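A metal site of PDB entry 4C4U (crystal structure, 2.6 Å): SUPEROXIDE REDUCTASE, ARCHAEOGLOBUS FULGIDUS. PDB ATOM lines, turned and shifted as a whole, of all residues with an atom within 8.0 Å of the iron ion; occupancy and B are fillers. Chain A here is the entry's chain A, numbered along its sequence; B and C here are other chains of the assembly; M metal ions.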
ATOM      1  N   LYS A  13      17.037  -6.233  15.225  1.00  0.00           N
ATOM      2  CA  LYS A  13      17.021  -7.613  14.739  1.00  0.00           C
ATOM      3  C   LYS A  13      16.999  -8.650  15.853  1.00  0.00           C
ATOM      4  O   LYS A  13      16.527  -9.778  15.662  1.00  0.00           O
ATOM      5  CB  LYS A  13      18.295  -7.822  13.897  1.00  0.00           C
ATOM      6  CG  LYS A  13      18.430  -9.155  13.205  1.00  0.00           C
ATOM      7  CD  LYS A  13      19.902  -9.364  12.816  1.00  0.00           C
ATOM      8  CE  LYS A  13      20.401  -8.486  11.671  1.00  0.00           C
ATOM      9  NZ  LYS A  13      19.901  -8.934  10.353  1.00  0.00           N
ATOM     10  N   HIS A  14      17.473  -8.254  17.022  1.00  0.00           N
ATOM     11  CA  HIS A  14      17.681  -9.177  18.118  1.00  0.00           C
ATOM     12  C   HIS A  14      16.648  -9.135  19.245  1.00  0.00           C
ATOM     13  O   HIS A  14      16.667  -9.999  20.130  1.00  0.00           O
ATOM     14  CB  HIS A  14      19.046  -8.937  18.748  1.00  0.00           C
ATOM     15  CG  HIS A  14      20.207  -9.413  17.931  1.00  0.00           C
ATOM     16  ND1 HIS A  14      20.982  -8.565  17.184  1.00  0.00           N
ATOM     17  CD2 HIS A  14      20.750 -10.653  17.793  1.00  0.00           C
ATOM     18  CE1 HIS A  14      21.947  -9.254  16.586  1.00  0.00           C
ATOM     19  NE2 HIS A  14      21.823 -10.524  16.938  1.00  0.00           N
ATOM     20  N   VAL A  34      12.430 -14.011  17.829  1.00  0.00           N
ATOM     21  CA  VAL A  34      13.545 -13.128  17.517  1.00  0.00           C
ATOM     22  C   VAL A  34      13.672 -13.019  16.012  1.00  0.00           C
ATOM     23  O   VAL A  34      13.785 -14.023  15.297  1.00  0.00           O
ATOM     24  CB  VAL A  34      14.876 -13.638  18.112  1.00  0.00           C
ATOM     25  CG1 VAL A  34      16.021 -12.836  17.583  1.00  0.00           C
ATOM     26  CG2 VAL A  34      14.846 -13.549  19.603  1.00  0.00           C
ATOM     27  N   HIS A  40      16.980 -12.611  11.471  1.00  0.00           N
ATOM     28  CA  HIS A  40      18.330 -12.761  11.993  1.00  0.00           C
ATOM     29  C   HIS A  40      18.962 -13.918  11.265  1.00  0.00           C
ATOM     30  O   HIS A  40      18.262 -14.858  10.879  1.00  0.00           O
ATOM     31  CB  HIS A  40      18.298 -13.051  13.495  1.00  0.00           C
ATOM     32  CG  HIS A  40      19.658 -13.111  14.131  1.00  0.00           C
ATOM     33  ND1 HIS A  40      20.485 -14.206  14.012  1.00  0.00           N
ATOM     34  CD2 HIS A  40      20.299 -12.222  14.922  1.00  0.00           C
ATOM     35  CE1 HIS A  40      21.600 -13.979  14.695  1.00  0.00           C
ATOM     36  NE2 HIS A  40      21.510 -12.788  15.250  1.00  0.00           N
ATOM     37  N   PRO A  41      20.278 -13.871  11.040  1.00  0.00           N
ATOM     38  CA  PRO A  41      20.860 -15.029  10.372  1.00  0.00           C
ATOM     39  C   PRO A  41      20.745 -16.281  11.229  1.00  0.00           C
ATOM     40  O   PRO A  41      20.619 -16.213  12.455  1.00  0.00           O
ATOM     41  CB  PRO A  41      22.336 -14.644  10.187  1.00  0.00           C
ATOM     42  CG  PRO A  41      22.345 -13.152  10.261  1.00  0.00           C
ATOM     43  CD  PRO A  41      21.248 -12.775  11.207  1.00  0.00           C
ATOM     44  N   GLU A  45      27.920 -20.309  12.171  1.00  0.00           N
ATOM     45  CA  GLU A  45      28.800 -19.295  12.755  1.00  0.00           C
ATOM     46  C   GLU A  45      28.030 -18.231  13.545  1.00  0.00           C
ATOM     47  O   GLU A  45      28.578 -17.640  14.486  1.00  0.00           O
ATOM     48  CB  GLU A  45      29.593 -18.623  11.649  1.00  0.00           C
ATOM     49  CG  GLU A  45      30.553 -19.587  10.952  1.00  0.00           C
ATOM     50  CD  GLU A  45      29.887 -20.364   9.822  1.00  0.00           C
ATOM     51  OE1 GLU A  45      28.814 -19.911   9.357  1.00  0.00           O
ATOM     52  OE2 GLU A  45      30.421 -21.433   9.449  1.00  0.00           O
ATOM     53  N   HIS A  46      26.771 -17.982  13.147  1.00  0.00           N
ATOM     54  CA  HIS A  46      25.950 -16.900  13.713  1.00  0.00           C
ATOM     55  C   HIS A  46      24.469 -17.323  13.796  1.00  0.00           C
ATOM     56  O   HIS A  46      23.877 -17.718  12.796  1.00  0.00           O
ATOM     57  CB  HIS A  46      26.106 -15.635  12.866  1.00  0.00           C
ATOM     58  CG  HIS A  46      25.364 -14.439  13.383  1.00  0.00           C
ATOM     59  ND1 HIS A  46      25.107 -13.330  12.602  1.00  0.00           N
ATOM     60  CD2 HIS A  46      24.834 -14.165  14.601  1.00  0.00           C
ATOM     61  CE1 HIS A  46      24.463 -12.425  13.320  1.00  0.00           C
ATOM     62  NE2 HIS A  46      24.279 -12.914  14.537  1.00  0.00           N
ATOM     63  N   HIS A  47      23.908 -17.286  15.004  1.00  0.00           N
ATOM     64  CA  HIS A  47      22.535 -17.770  15.208  1.00  0.00           C
ATOM     65  C   HIS A  47      21.944 -17.418  16.566  1.00  0.00           C
ATOM     66  O   HIS A  47      22.674 -17.280  17.561  1.00  0.00           O
ATOM     67  CB  HIS A  47      22.480 -19.302  15.042  1.00  0.00           C
ATOM     68  CG  HIS A  47      23.514 -20.029  15.874  1.00  0.00           C
ATOM     69  ND1 HIS A  47      24.582 -20.693  15.312  1.00  0.00           N
ATOM     70  CD2 HIS A  47      23.666 -20.140  17.206  1.00  0.00           C
ATOM     71  CE1 HIS A  47      25.337 -21.196  16.267  1.00  0.00           C
ATOM     72  NE2 HIS A  47      24.800 -20.873  17.435  1.00  0.00           N
ATOM     73  N   ILE A  48      20.617 -17.327  16.619  1.00  0.00           N
ATOM     74  CA  ILE A  48      19.934 -17.222  17.919  1.00  0.00           C
ATOM     75  C   ILE A  48      19.844 -18.599  18.553  1.00  0.00           C
ATOM     76  O   ILE A  48      19.449 -19.569  17.912  1.00  0.00           O
ATOM     77  CB  ILE A  48      18.519 -16.607  17.790  1.00  0.00           C
ATOM     78  CG1 ILE A  48      18.621 -15.206  17.173  1.00  0.00           C
ATOM     79  CG2 ILE A  48      17.869 -16.479  19.157  1.00  0.00           C
ATOM     80  CD1 ILE A  48      19.386 -14.170  18.051  1.00  0.00           C
ATOM     81  N   TYR A 109      19.143 -15.030  23.335  1.00  0.00           N
ATOM     82  CA  TYR A 109      20.576 -15.053  23.311  1.00  0.00           C
ATOM     83  C   TYR A 109      21.077 -15.270  21.898  1.00  0.00           C
ATOM     84  O   TYR A 109      20.675 -16.199  21.200  1.00  0.00           O
ATOM     85  CB  TYR A 109      21.108 -16.144  24.253  1.00  0.00           C
ATOM     86  CG  TYR A 109      22.607 -16.234  24.295  1.00  0.00           C
ATOM     87  CD1 TYR A 109      23.359 -15.156  24.722  1.00  0.00           C
ATOM     88  CD2 TYR A 109      23.275 -17.371  23.843  1.00  0.00           C
ATOM     89  CE1 TYR A 109      24.721 -15.200  24.754  1.00  0.00           C
ATOM     90  CE2 TYR A 109      24.646 -17.424  23.868  1.00  0.00           C
ATOM     91  CZ  TYR A 109      25.360 -16.324  24.322  1.00  0.00           C
ATOM     92  OH  TYR A 109      26.725 -16.333  24.355  1.00  0.00           O
ATOM     93  N   CYS A 110      21.932 -14.362  21.468  1.00  0.00           N
ATOM     94  CA  CYS A 110      22.687 -14.588  20.257  1.00  0.00           C
ATOM     95  C   CYS A 110      24.070 -15.032  20.668  1.00  0.00           C
ATOM     96  O   CYS A 110      24.601 -14.528  21.646  1.00  0.00           O
ATOM     97  CB  CYS A 110      22.805 -13.304  19.423  1.00  0.00           C
ATOM     98  SG  CYS A 110      23.848 -13.513  17.942  1.00  0.00           S
ATOM     99  N   ASN A 111      24.627 -16.008  19.957  1.00  0.00           N
ATOM    100  CA  ASN A 111      25.967 -16.482  20.295  1.00  0.00           C
ATOM    101  C   ASN A 111      27.058 -15.427  20.056  1.00  0.00           C
ATOM    102  O   ASN A 111      28.127 -15.488  20.666  1.00  0.00           O
ATOM    103  CB  ASN A 111      26.305 -17.781  19.563  1.00  0.00           C
ATOM    104  CG  ASN A 111      26.582 -17.572  18.088  1.00  0.00           C
ATOM    105  OD1 ASN A 111      26.114 -16.599  17.472  1.00  0.00           O
ATOM    106  ND2 ASN A 111      27.325 -18.507  17.501  1.00  0.00           N
ATOM    107  N   ILE A 112      26.809 -14.439  19.202  1.00  0.00           N
ATOM    108  CA  ILE A 112      27.839 -13.424  19.079  1.00  0.00           C
ATOM    109  C   ILE A 112      27.384 -12.018  19.438  1.00  0.00           C
ATOM    110  O   ILE A 112      28.215 -11.155  19.690  1.00  0.00           O
ATOM    111  CB  ILE A 112      28.520 -13.419  17.661  1.00  0.00           C
ATOM    112  CG1 ILE A 112      27.587 -12.865  16.574  1.00  0.00           C
ATOM    113  CG2 ILE A 112      29.015 -14.819  17.271  1.00  0.00           C
ATOM    114  CD1 ILE A 112      28.187 -12.882  15.198  1.00  0.00           C
ATOM    115  N   HIS A 113      26.092 -11.773  19.566  1.00  0.00           N
ATOM    116  CA  HIS A 113      25.662 -10.403  19.851  1.00  0.00           C
ATOM    117  C   HIS A 113      25.033 -10.261  21.230  1.00  0.00           C
ATOM    118  O   HIS A 113      24.243  -9.349  21.478  1.00  0.00           O
ATOM    119  CB  HIS A 113      24.710  -9.853  18.773  1.00  0.00           C
ATOM    120  CG  HIS A 113      25.356  -9.565  17.446  1.00  0.00           C
ATOM    121  ND1 HIS A 113      25.020 -10.230  16.288  1.00  0.00           N
ATOM    122  CD2 HIS A 113      26.312  -8.672  17.109  1.00  0.00           C
ATOM    123  CE1 HIS A 113      25.739  -9.750  15.286  1.00  0.00           C
ATOM    124  NE2 HIS A 113      26.530  -8.805  15.755  1.00  0.00           N
ATOM    125  N   GLY A 114      25.389 -11.181  22.114  1.00  0.00           N
ATOM    126  CA  GLY A 114      25.028 -11.080  23.512  1.00  0.00           C
ATOM    127  C   GLY A 114      23.563 -11.355  23.801  1.00  0.00           C
ATOM    128  O   GLY A 114      22.861 -12.027  23.027  1.00  0.00           O
ATOM    129  N   TRP A 116      19.558 -10.426  25.094  1.00  0.00           N
ATOM    130  CA  TRP A 116      18.522  -9.454  24.745  1.00  0.00           C
ATOM    131  C   TRP A 116      17.241  -9.675  25.549  1.00  0.00           C
ATOM    132  O   TRP A 116      16.970 -10.795  25.989  1.00  0.00           O
ATOM    133  CB  TRP A 116      18.230  -9.540  23.241  1.00  0.00           C
ATOM    134  CG  TRP A 116      19.412  -9.195  22.398  1.00  0.00           C
ATOM    135  CD1 TRP A 116      20.471 -10.006  22.075  1.00  0.00           C
ATOM    136  CD2 TRP A 116      19.660  -7.951  21.738  1.00  0.00           C
ATOM    137  NE1 TRP A 116      21.360  -9.336  21.267  1.00  0.00           N
ATOM    138  CE2 TRP A 116      20.884  -8.066  21.047  1.00  0.00           C
ATOM    139  CE3 TRP A 116      18.940  -6.740  21.650  1.00  0.00           C
ATOM    140  CZ2 TRP A 116      21.412  -7.037  20.271  1.00  0.00           C
ATOM    141  CZ3 TRP A 116      19.479  -5.713  20.909  1.00  0.00           C
ATOM    142  CH2 TRP A 116      20.700  -5.862  20.231  1.00  0.00           C
ATOM    143  N   VAL B  78      31.884 -11.595  16.651  1.00  0.00           N
ATOM    144  CA  VAL B  78      31.662 -10.716  15.498  1.00  0.00           C
ATOM    145  C   VAL B  78      32.826 -10.768  14.504  1.00  0.00           C
ATOM    146  O   VAL B  78      32.639 -10.520  13.330  1.00  0.00           O
ATOM    147  CB  VAL B  78      31.495  -9.233  15.901  1.00  0.00           C
ATOM    148  CG1 VAL B  78      30.259  -9.051  16.774  1.00  0.00           C
ATOM    149  CG2 VAL B  78      32.744  -8.730  16.628  1.00  0.00           C
ATOM    150  N   PHE C  62      30.412  -7.649  23.380  1.00  0.00           N
ATOM    151  CA  PHE C  62      29.329  -8.527  23.783  1.00  0.00           C
ATOM    152  C   PHE C  62      29.836  -9.567  24.760  1.00  0.00           C
ATOM    153  O   PHE C  62      30.998  -9.935  24.735  1.00  0.00           O
ATOM    154  CB  PHE C  62      28.692  -9.166  22.543  1.00  0.00           C
ATOM    155  CG  PHE C  62      28.162  -8.160  21.565  1.00  0.00           C
ATOM    156  CD1 PHE C  62      26.957  -7.510  21.803  1.00  0.00           C
ATOM    157  CD2 PHE C  62      28.887  -7.813  20.420  1.00  0.00           C
ATOM    158  CE1 PHE C  62      26.462  -6.566  20.906  1.00  0.00           C
ATOM    159  CE2 PHE C  62      28.403  -6.861  19.528  1.00  0.00           C
ATOM    160  CZ  PHE C  62      27.186  -6.238  19.771  1.00  0.00           C
HETATM  161 FE    FE M   1      23.414 -11.965  16.286  1.00  0.00          FE
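N of Ile 112 sits close to SG of Cys 110 (3.3 Å). O of His 113 lies within hydrogen-bond range of NE1 of Trp 116, at 2.9 Å.
Five residues have an atom within 4 Å of the iron ion: His 14, His 40, His 46, Cys 110 and His 113.
The iron ion is bound by a ring nitrogen (NE2) of His 46, a ring nitrogen (NE2) of His 14, the side-chain sulfur of Cys 110, a ring nitrogen (NE2) of His 40 and a ring nitrogen (ND1) of His 113.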
